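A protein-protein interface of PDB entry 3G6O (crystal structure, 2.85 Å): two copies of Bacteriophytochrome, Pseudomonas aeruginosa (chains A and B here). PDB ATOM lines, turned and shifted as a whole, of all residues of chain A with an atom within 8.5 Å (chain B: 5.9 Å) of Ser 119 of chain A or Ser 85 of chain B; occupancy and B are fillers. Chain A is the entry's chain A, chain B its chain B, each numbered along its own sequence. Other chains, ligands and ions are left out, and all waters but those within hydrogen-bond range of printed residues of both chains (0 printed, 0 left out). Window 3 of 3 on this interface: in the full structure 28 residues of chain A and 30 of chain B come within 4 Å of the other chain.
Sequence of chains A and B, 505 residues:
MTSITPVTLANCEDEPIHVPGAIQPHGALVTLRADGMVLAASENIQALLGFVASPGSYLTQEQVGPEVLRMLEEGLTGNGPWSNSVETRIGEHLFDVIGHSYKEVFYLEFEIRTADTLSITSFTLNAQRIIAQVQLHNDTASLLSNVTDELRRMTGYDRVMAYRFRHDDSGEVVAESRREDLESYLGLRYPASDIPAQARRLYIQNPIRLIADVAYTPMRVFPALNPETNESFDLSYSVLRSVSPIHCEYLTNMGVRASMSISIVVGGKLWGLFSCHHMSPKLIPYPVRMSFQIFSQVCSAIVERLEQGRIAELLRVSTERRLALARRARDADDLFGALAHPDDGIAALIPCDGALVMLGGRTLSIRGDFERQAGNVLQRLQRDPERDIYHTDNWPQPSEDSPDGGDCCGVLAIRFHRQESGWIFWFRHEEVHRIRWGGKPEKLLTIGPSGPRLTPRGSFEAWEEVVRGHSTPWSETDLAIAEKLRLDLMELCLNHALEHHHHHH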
ATOM      1  N   GLU A  87       9.425 -19.573   3.163  1.00  0.00           N
ATOM      2  CA  GLU A  87      10.550 -20.469   3.368  1.00  0.00           C
ATOM      3  C   GLU A  87      10.031 -21.703   4.070  1.00  0.00           C
ATOM      4  O   GLU A  87       9.844 -21.703   5.285  1.00  0.00           O
ATOM      5  CB  GLU A  87      11.596 -19.776   4.228  1.00  0.00           C
ATOM      6  CG  GLU A  87      13.008 -19.913   3.731  1.00  0.00           C
ATOM      7  CD  GLU A  87      13.879 -18.765   4.199  1.00  0.00           C
ATOM      8  OE1 GLU A  87      14.501 -18.898   5.274  1.00  0.00           O
ATOM      9  OE2 GLU A  87      13.921 -17.721   3.506  1.00  0.00           O
ATOM     10  N   ARG A 113      17.022 -23.983  -1.004  1.00  0.00           N
ATOM     11  CA  ARG A 113      17.657 -23.178   0.022  1.00  0.00           C
ATOM     12  C   ARG A 113      18.826 -23.890   0.702  1.00  0.00           C
ATOM     13  O   ARG A 113      18.791 -25.098   0.952  1.00  0.00           O
ATOM     14  CB  ARG A 113      16.637 -22.720   1.068  1.00  0.00           C
ATOM     15  CG  ARG A 113      17.240 -21.815   2.132  1.00  0.00           C
ATOM     16  CD  ARG A 113      16.197 -20.984   2.846  1.00  0.00           C
ATOM     17  NE  ARG A 113      16.786 -19.839   3.531  1.00  0.00           N
ATOM     18  CZ  ARG A 113      17.029 -18.672   2.945  1.00  0.00           C
ATOM     19  NH1 ARG A 113      16.735 -18.499   1.662  1.00  0.00           N
ATOM     20  NH2 ARG A 113      17.564 -17.680   3.640  1.00  0.00           N
ATOM     21  N   ASP A 116      21.566 -20.112   6.483  1.00  0.00           N
ATOM     22  CA  ASP A 116      20.273 -20.046   7.167  1.00  0.00           C
ATOM     23  C   ASP A 116      19.485 -18.827   6.718  1.00  0.00           C
ATOM     24  O   ASP A 116      19.845 -18.149   5.752  1.00  0.00           O
ATOM     25  CB  ASP A 116      20.470 -19.903   8.678  1.00  0.00           C
ATOM     26  CG  ASP A 116      20.525 -21.231   9.398  1.00  0.00           C
ATOM     27  OD1 ASP A 116      19.651 -22.089   9.151  1.00  0.00           O
ATOM     28  OD2 ASP A 116      21.434 -21.404  10.240  1.00  0.00           O
ATOM     29  N   THR A 117      18.421 -18.534   7.461  1.00  0.00           N
ATOM     30  CA  THR A 117      17.572 -17.377   7.199  1.00  0.00           C
ATOM     31  C   THR A 117      18.347 -16.071   7.232  1.00  0.00           C
ATOM     32  O   THR A 117      18.945 -15.711   8.242  1.00  0.00           O
ATOM     33  CB  THR A 117      16.422 -17.269   8.226  1.00  0.00           C
ATOM     34  OG1 THR A 117      15.820 -18.557   8.404  1.00  0.00           O
ATOM     35  CG2 THR A 117      15.363 -16.250   7.762  1.00  0.00           C
ATOM     36  N   LEU A 118      18.333 -15.366   6.111  1.00  0.00           N
ATOM     37  CA  LEU A 118      18.779 -13.988   6.084  1.00  0.00           C
ATOM     38  C   LEU A 118      17.855 -13.206   6.995  1.00  0.00           C
ATOM     39  O   LEU A 118      16.654 -13.086   6.727  1.00  0.00           O
ATOM     40  CB  LEU A 118      18.684 -13.422   4.668  1.00  0.00           C
ATOM     41  CG  LEU A 118      19.586 -12.233   4.342  1.00  0.00           C
ATOM     42  CD1 LEU A 118      21.034 -12.693   4.194  1.00  0.00           C
ATOM     43  CD2 LEU A 118      19.110 -11.511   3.083  1.00  0.00           C
ATOM     44  N   SER A 119      18.404 -12.697   8.091  1.00  0.00           N
ATOM     45  CA  SER A 119      17.648 -11.810   8.951  1.00  0.00           C
ATOM     46  C   SER A 119      17.147 -10.698   8.061  1.00  0.00           C
ATOM     47  O   SER A 119      17.806 -10.335   7.089  1.00  0.00           O
ATOM     48  CB  SER A 119      18.558 -11.212  10.014  1.00  0.00           C
ATOM     49  OG  SER A 119      19.644 -12.087  10.291  1.00  0.00           O
ATOM     50  N   ILE A 120      15.979 -10.166   8.382  1.00  0.00           N
ATOM     51  CA  ILE A 120      15.475  -8.978   7.711  1.00  0.00           C
ATOM     52  C   ILE A 120      16.537  -7.893   7.760  1.00  0.00           C
ATOM     53  O   ILE A 120      16.740  -7.139   6.808  1.00  0.00           O
ATOM     54  CB  ILE A 120      14.274  -8.412   8.455  1.00  0.00           C
ATOM     55  CG1 ILE A 120      13.891  -9.318   9.647  1.00  0.00           C
ATOM     56  CG2 ILE A 120      13.144  -8.130   7.476  1.00  0.00           C
ATOM     57  CD1 ILE A 120      13.436 -10.744   9.295  1.00  0.00           C
ATOM     58  N   THR A 121      17.194  -7.818   8.909  1.00  0.00           N
ATOM     59  CA  THR A 121      18.212  -6.821   9.171  1.00  0.00           C
ATOM     60  C   THR A 121      19.420  -7.048   8.271  1.00  0.00           C
ATOM     61  O   THR A 121      19.869  -6.123   7.600  1.00  0.00           O
ATOM     62  CB  THR A 121      18.648  -6.860  10.649  1.00  0.00           C
ATOM     63  OG1 THR A 121      17.497  -7.058  11.481  1.00  0.00           O
ATOM     64  CG2 THR A 121      19.313  -5.565  11.035  1.00  0.00           C
ATOM     65  N   SER A 122      19.941  -8.276   8.260  1.00  0.00           N
ATOM     66  CA  SER A 122      21.055  -8.639   7.388  1.00  0.00           C
ATOM     67  C   SER A 122      20.692  -8.260   5.954  1.00  0.00           C
ATOM     68  O   SER A 122      21.530  -7.766   5.193  1.00  0.00           O
ATOM     69  CB  SER A 122      21.330 -10.140   7.452  1.00  0.00           C
ATOM     70  OG  SER A 122      21.568 -10.577   8.775  1.00  0.00           O
ATOM     71  N   PHE A 123      19.431  -8.493   5.592  1.00  0.00           N
ATOM     72  CA  PHE A 123      18.944  -8.140   4.271  1.00  0.00           C
ATOM     73  C   PHE A 123      18.940  -6.624   4.050  1.00  0.00           C
ATOM     74  O   PHE A 123      19.296  -6.152   2.973  1.00  0.00           O
ATOM     75  CB  PHE A 123      17.550  -8.719   4.042  1.00  0.00           C
ATOM     76  CG  PHE A 123      16.880  -8.203   2.804  1.00  0.00           C
ATOM     77  CD1 PHE A 123      17.048  -8.850   1.594  1.00  0.00           C
ATOM     78  CD2 PHE A 123      16.081  -7.074   2.850  1.00  0.00           C
ATOM     79  CE1 PHE A 123      16.429  -8.374   0.450  1.00  0.00           C
ATOM     80  CE2 PHE A 123      15.464  -6.598   1.717  1.00  0.00           C
ATOM     81  CZ  PHE A 123      15.636  -7.247   0.516  1.00  0.00           C
ATOM     82  N   THR A 124      18.534  -5.862   5.062  1.00  0.00           N
ATOM     83  CA  THR A 124      18.461  -4.412   4.913  1.00  0.00           C
ATOM     84  C   THR A 124      19.835  -3.761   4.723  1.00  0.00           C
ATOM     85  O   THR A 124      19.948  -2.770   3.990  1.00  0.00           O
ATOM     86  CB  THR A 124      17.703  -3.721   6.063  1.00  0.00           C
ATOM     87  OG1 THR A 124      16.387  -4.279   6.167  1.00  0.00           O
ATOM     88  CG2 THR A 124      17.603  -2.211   5.811  1.00  0.00           C
ATOM     89  N   LEU A 125      20.882  -4.294   5.356  1.00  0.00           N
ATOM     90  CA  LEU A 125      22.195  -3.692   5.126  1.00  0.00           C
ATOM     91  C   LEU A 125      22.997  -4.291   3.965  1.00  0.00           C
ATOM     92  O   LEU A 125      24.028  -3.747   3.579  1.00  0.00           O
ATOM     93  CB  LEU A 125      23.031  -3.514   6.398  1.00  0.00           C
ATOM     94  CG  LEU A 125      23.971  -2.321   6.123  1.00  0.00           C
ATOM     95  CD1 LEU A 125      23.965  -1.277   7.238  1.00  0.00           C
ATOM     96  CD2 LEU A 125      25.406  -2.751   5.766  1.00  0.00           C
ATOM     97  N   ASN A 126      22.522  -5.383   3.379  1.00  0.00           N
ATOM     98  CA  ASN A 126      23.043  -5.739   2.065  1.00  0.00           C
ATOM     99  C   ASN A 126      22.572  -4.704   1.061  1.00  0.00           C
ATOM    100  O   ASN A 126      23.371  -4.127   0.323  1.00  0.00           O
ATOM    101  CB  ASN A 126      22.647  -7.145   1.631  1.00  0.00           C
ATOM    102  CG  ASN A 126      23.828  -8.093   1.616  1.00  0.00           C
ATOM    103  OD1 ASN A 126      24.638  -8.106   2.546  1.00  0.00           O
ATOM    104  ND2 ASN A 126      23.945  -8.880   0.552  1.00  0.00           N
ATOM    105  N   PRO A 287      16.573 -14.281  -1.510  1.00  0.00           N
ATOM    106  CA  PRO A 287      16.565 -13.071  -0.685  1.00  0.00           C
ATOM    107  C   PRO A 287      17.616 -12.082  -1.141  1.00  0.00           C
ATOM    108  O   PRO A 287      17.334 -10.888  -1.226  1.00  0.00           O
ATOM    109  CB  PRO A 287      16.917 -13.602   0.699  1.00  0.00           C
ATOM    110  CG  PRO A 287      16.366 -14.981   0.712  1.00  0.00           C
ATOM    111  CD  PRO A 287      16.584 -15.502  -0.686  1.00  0.00           C
ATOM    112  N   MET B  71      22.078 -15.827  17.472  1.00  0.00           N
ATOM    113  CA  MET B  71      22.267 -14.453  17.049  1.00  0.00           C
ATOM    114  C   MET B  71      23.339 -13.815  17.906  1.00  0.00           C
ATOM    115  O   MET B  71      24.435 -13.515  17.432  1.00  0.00           O
ATOM    116  CB  MET B  71      20.969 -13.680  17.232  1.00  0.00           C
ATOM    117  CG  MET B  71      21.114 -12.186  17.118  1.00  0.00           C
ATOM    118  SD  MET B  71      19.510 -11.414  16.834  1.00  0.00           S
ATOM    119  CE  MET B  71      19.049 -10.933  18.494  1.00  0.00           C
ATOM    120  N   GLU B  74      26.900 -14.724  17.289  1.00  0.00           N
ATOM    121  CA  GLU B  74      27.505 -14.215  16.071  1.00  0.00           C
ATOM    122  C   GLU B  74      27.872 -12.757  16.292  1.00  0.00           C
ATOM    123  O   GLU B  74      28.709 -12.204  15.590  1.00  0.00           O
ATOM    124  CB  GLU B  74      26.595 -14.409  14.851  1.00  0.00           C
ATOM    125  CG  GLU B  74      25.481 -13.403  14.689  1.00  0.00           C
ATOM    126  CD  GLU B  74      24.729 -13.595  13.385  1.00  0.00           C
ATOM    127  OE1 GLU B  74      25.244 -13.164  12.329  1.00  0.00           O
ATOM    128  OE2 GLU B  74      23.622 -14.177  13.417  1.00  0.00           O
ATOM    129  N   SER B  83      24.771  -5.398  14.122  1.00  0.00           N
ATOM    130  CA  SER B  83      23.357  -5.108  13.999  1.00  0.00           C
ATOM    131  C   SER B  83      22.690  -6.353  13.464  1.00  0.00           C
ATOM    132  O   SER B  83      23.202  -6.991  12.540  1.00  0.00           O
ATOM    133  CB  SER B  83      23.117  -3.953  13.046  1.00  0.00           C
ATOM    134  OG  SER B  83      21.807  -3.436  13.225  1.00  0.00           O
ATOM    135  N   ASN B  84      21.558  -6.720  14.047  1.00  0.00           N
ATOM    136  CA  ASN B  84      20.861  -7.914  13.591  1.00  0.00           C
ATOM    137  C   ASN B  84      19.619  -8.173  14.401  1.00  0.00           C
ATOM    138  O   ASN B  84      19.375  -7.491  15.396  1.00  0.00           O
ATOM    139  CB  ASN B  84      21.781  -9.138  13.651  1.00  0.00           C
ATOM    140  CG  ASN B  84      21.341 -10.237  12.700  1.00  0.00           C
ATOM    141  OD1 ASN B  84      20.319 -10.107  12.033  1.00  0.00           O
ATOM    142  ND2 ASN B  84      22.114 -11.320  12.626  1.00  0.00           N
ATOM    143  N   SER B  85      18.854  -9.177  13.993  1.00  0.00           N
ATOM    144  CA  SER B  85      17.599  -9.496  14.661  1.00  0.00           C
ATOM    145  C   SER B  85      17.063 -10.844  14.220  1.00  0.00           C
ATOM    146  O   SER B  85      17.504 -11.414  13.216  1.00  0.00           O
ATOM    147  CB  SER B  85      16.540  -8.437  14.381  1.00  0.00           C
ATOM    148  OG  SER B  85      15.991  -8.630  13.095  1.00  0.00           O
ATOM    149  N   VAL B  86      16.075 -11.324  14.965  1.00  0.00           N
ATOM    150  CA  VAL B  86      15.552 -12.670  14.798  1.00  0.00           C
ATOM    151  C   VAL B  86      14.145 -12.748  15.355  1.00  0.00           C
ATOM    152  O   VAL B  86      13.819 -12.097  16.349  1.00  0.00           O
ATOM    153  CB  VAL B  86      16.449 -13.699  15.500  1.00  0.00           C
ATOM    154  CG1 VAL B  86      15.661 -14.517  16.501  1.00  0.00           C
ATOM    155  CG2 VAL B  86      17.144 -14.579  14.477  1.00  0.00           C
ATOM    156  N   GLU B  87      13.310 -13.551  14.710  1.00  0.00           N
ATOM    157  CA  GLU B  87      11.903 -13.621  15.066  1.00  0.00           C
ATOM    158  C   GLU B  87      11.636 -14.873  15.879  1.00  0.00           C
ATOM    159  O   GLU B  87      11.083 -15.847  15.379  1.00  0.00           O
ATOM    160  CB  GLU B  87      11.055 -13.622  13.801  1.00  0.00           C
ATOM    161  CG  GLU B  87       9.649 -13.101  13.968  1.00  0.00           C
ATOM    162  CD  GLU B  87       9.032 -12.729  12.635  1.00  0.00           C
ATOM    163  OE1 GLU B  87       8.043 -13.380  12.236  1.00  0.00           O
ATOM    164  OE2 GLU B  87       9.547 -11.795  11.977  1.00  0.00           O
ATOM    165  N   ASP B  96       9.985  -9.996  18.005  1.00  0.00           N
ATOM    166  CA  ASP B  96      11.055  -9.399  17.211  1.00  0.00           C
ATOM    167  C   ASP B  96      12.190  -9.010  18.159  1.00  0.00           C
ATOM    168  O   ASP B  96      12.062  -8.057  18.930  1.00  0.00           O
ATOM    169  CB  ASP B  96      10.558  -8.136  16.513  1.00  0.00           C
ATOM    170  CG  ASP B  96      10.202  -8.366  15.058  1.00  0.00           C
ATOM    171  OD1 ASP B  96      10.857  -9.212  14.402  1.00  0.00           O
ATOM    172  OD2 ASP B  96       9.277  -7.673  14.568  1.00  0.00           O
ATOM    173  N   VAL B  97      13.300  -9.739  18.113  1.00  0.00           N
ATOM    174  CA  VAL B  97      14.408  -9.472  19.020  1.00  0.00           C
ATOM    175  C   VAL B  97      15.531  -8.715  18.305  1.00  0.00           C
ATOM    176  O   VAL B  97      16.319  -9.297  17.560  1.00  0.00           O
ATOM    177  CB  VAL B  97      14.923 -10.778  19.665  1.00  0.00           C
ATOM    178  CG1 VAL B  97      16.331 -10.614  20.211  1.00  0.00           C
ATOM    179  CG2 VAL B  97      13.971 -11.233  20.745  1.00  0.00           C
ATOM    180  N   ILE B  98      15.600  -7.412  18.547  1.00  0.00           N
ATOM    181  CA  ILE B  98      16.512  -6.545  17.812  1.00  0.00           C
ATOM    182  C   ILE B  98      17.749  -6.206  18.649  1.00  0.00           C
ATOM    183  O   ILE B  98      17.650  -5.742  19.786  1.00  0.00           O
ATOM    184  CB  ILE B  98      15.792  -5.263  17.362  1.00  0.00           C
ATOM    185  CG1 ILE B  98      15.720  -4.251  18.504  1.00  0.00           C
ATOM    186  CG2 ILE B  98      14.378  -5.586  16.888  1.00  0.00           C
ATOM    187  CD1 ILE B  98      14.472  -3.404  18.490  1.00  0.00           C
ATOM    188  N   GLY B  99      18.924  -6.449  18.087  1.00  0.00           N
ATOM    189  CA  GLY B  99      20.153  -6.241  18.825  1.00  0.00           C
ATOM    190  C   GLY B  99      21.157  -5.397  18.076  1.00  0.00           C
ATOM    191  O   GLY B  99      21.173  -5.376  16.841  1.00  0.00           O
ATOM    192  N   TYR B 286       9.021  -3.716  13.397  1.00  0.00           N
ATOM    193  CA  TYR B 286      10.429  -3.572  13.016  1.00  0.00           C
ATOM    194  C   TYR B 286      10.616  -3.648  11.503  1.00  0.00           C
ATOM    195  O   TYR B 286      11.046  -2.675  10.879  1.00  0.00           O
ATOM    196  CB  TYR B 286      11.298  -4.638  13.705  1.00  0.00           C
ATOM    197  CG  TYR B 286      12.783  -4.528  13.425  1.00  0.00           C
ATOM    198  CD1 TYR B 286      13.531  -3.487  13.956  1.00  0.00           C
ATOM    199  CD2 TYR B 286      13.442  -5.475  12.645  1.00  0.00           C
ATOM    200  CE1 TYR B 286      14.887  -3.379  13.704  1.00  0.00           C
ATOM    201  CE2 TYR B 286      14.809  -5.375  12.393  1.00  0.00           C
ATOM    202  CZ  TYR B 286      15.521  -4.323  12.924  1.00  0.00           C
ATOM    203  OH  TYR B 286      16.872  -4.204  12.681  1.00  0.00           O
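OG1 of Thr 121 of chain A is in hydrogen-bond range of OG of Ser 85 of chain B, at 2.7 Å. The side-chain hydroxyl (OG1) of Thr 121 of chain A sits at hydrogen-bond distance from the side-chain hydroxyl (OH) of Tyr 286 of chain B (3.2 Å). The side-chain hydroxyl (OG) of Ser 119 of chain A lies within hydrogen-bond range of the side-chain amide oxygen (OD1) of Asn 84 of chain B, 2.7 Å away.
Hydrophobic or aromatic side chains of chain B within 4 Å of the printed part of chain A: Tyr 286. Along chain B the printed residues that touch a printed residue of chain A span positions 83 to 286.
Among the printed residues, pairs that only touch across the chains: Ser 119 of chain A with Ser 85 of chain B, Ser 122 of chain A with Asn 84 of chain B, Thr 121 of chain A with Asn 84 of chain B and Thr 121 of chain A with Ser 83 of chain B.
Position printed for both chains: 87. Of the 7 pairs that touch across the chains among the printed residues, none has its exchanged pair printed and touching as well.
Of chain B, only Asn 84 and Ser 85 come within 4 Å of Ser 119 of chain A. Of chain A, only Ser 119 and Thr 121 come within 4 Å of Ser 85 of chain B. Asn 84 of chain B touches just these residues of chain A: Ser 119, Thr 121 and Ser 122. Printed residues of chain A within 4 Å of Tyr 286 of chain B: Thr 121. Printed residues of chain B within 4 Å of Thr 121 of chain A: Ser 83, Asn 84, Ser 85 and Tyr 286. Of the printed residues of chain B, Ser 122 of chain A touches Asn 84 (3.5 Å). Of the printed residues of chain A, Ser 83 of chain B touches Thr 121. Thr 117 of chain A touches none of the printed residues of chain B. Glu 87 of chain A touches none of the printed residues of chain B. The nearest printed residue of chain B that does not touch Ser 119 of chain A is Glu 74 of chain B (5.5 Å).
OG of Ser 119 of chain A is in hydrogen-bond range of OG of Ser 122 of chain A (2.9 Å). N of Gly 99 of chain B is in hydrogen-bond range of O of Asn 84 of chain B, at 2.9 Å. OE2 of Glu 74 of chain B sits at hydrogen-bond distance from ND2 of Asn 84 of chain B. The backbone NH of Ser 85 of chain B sits close to the side-chain sulfur of Met 71 of chain B (3.7 Å).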
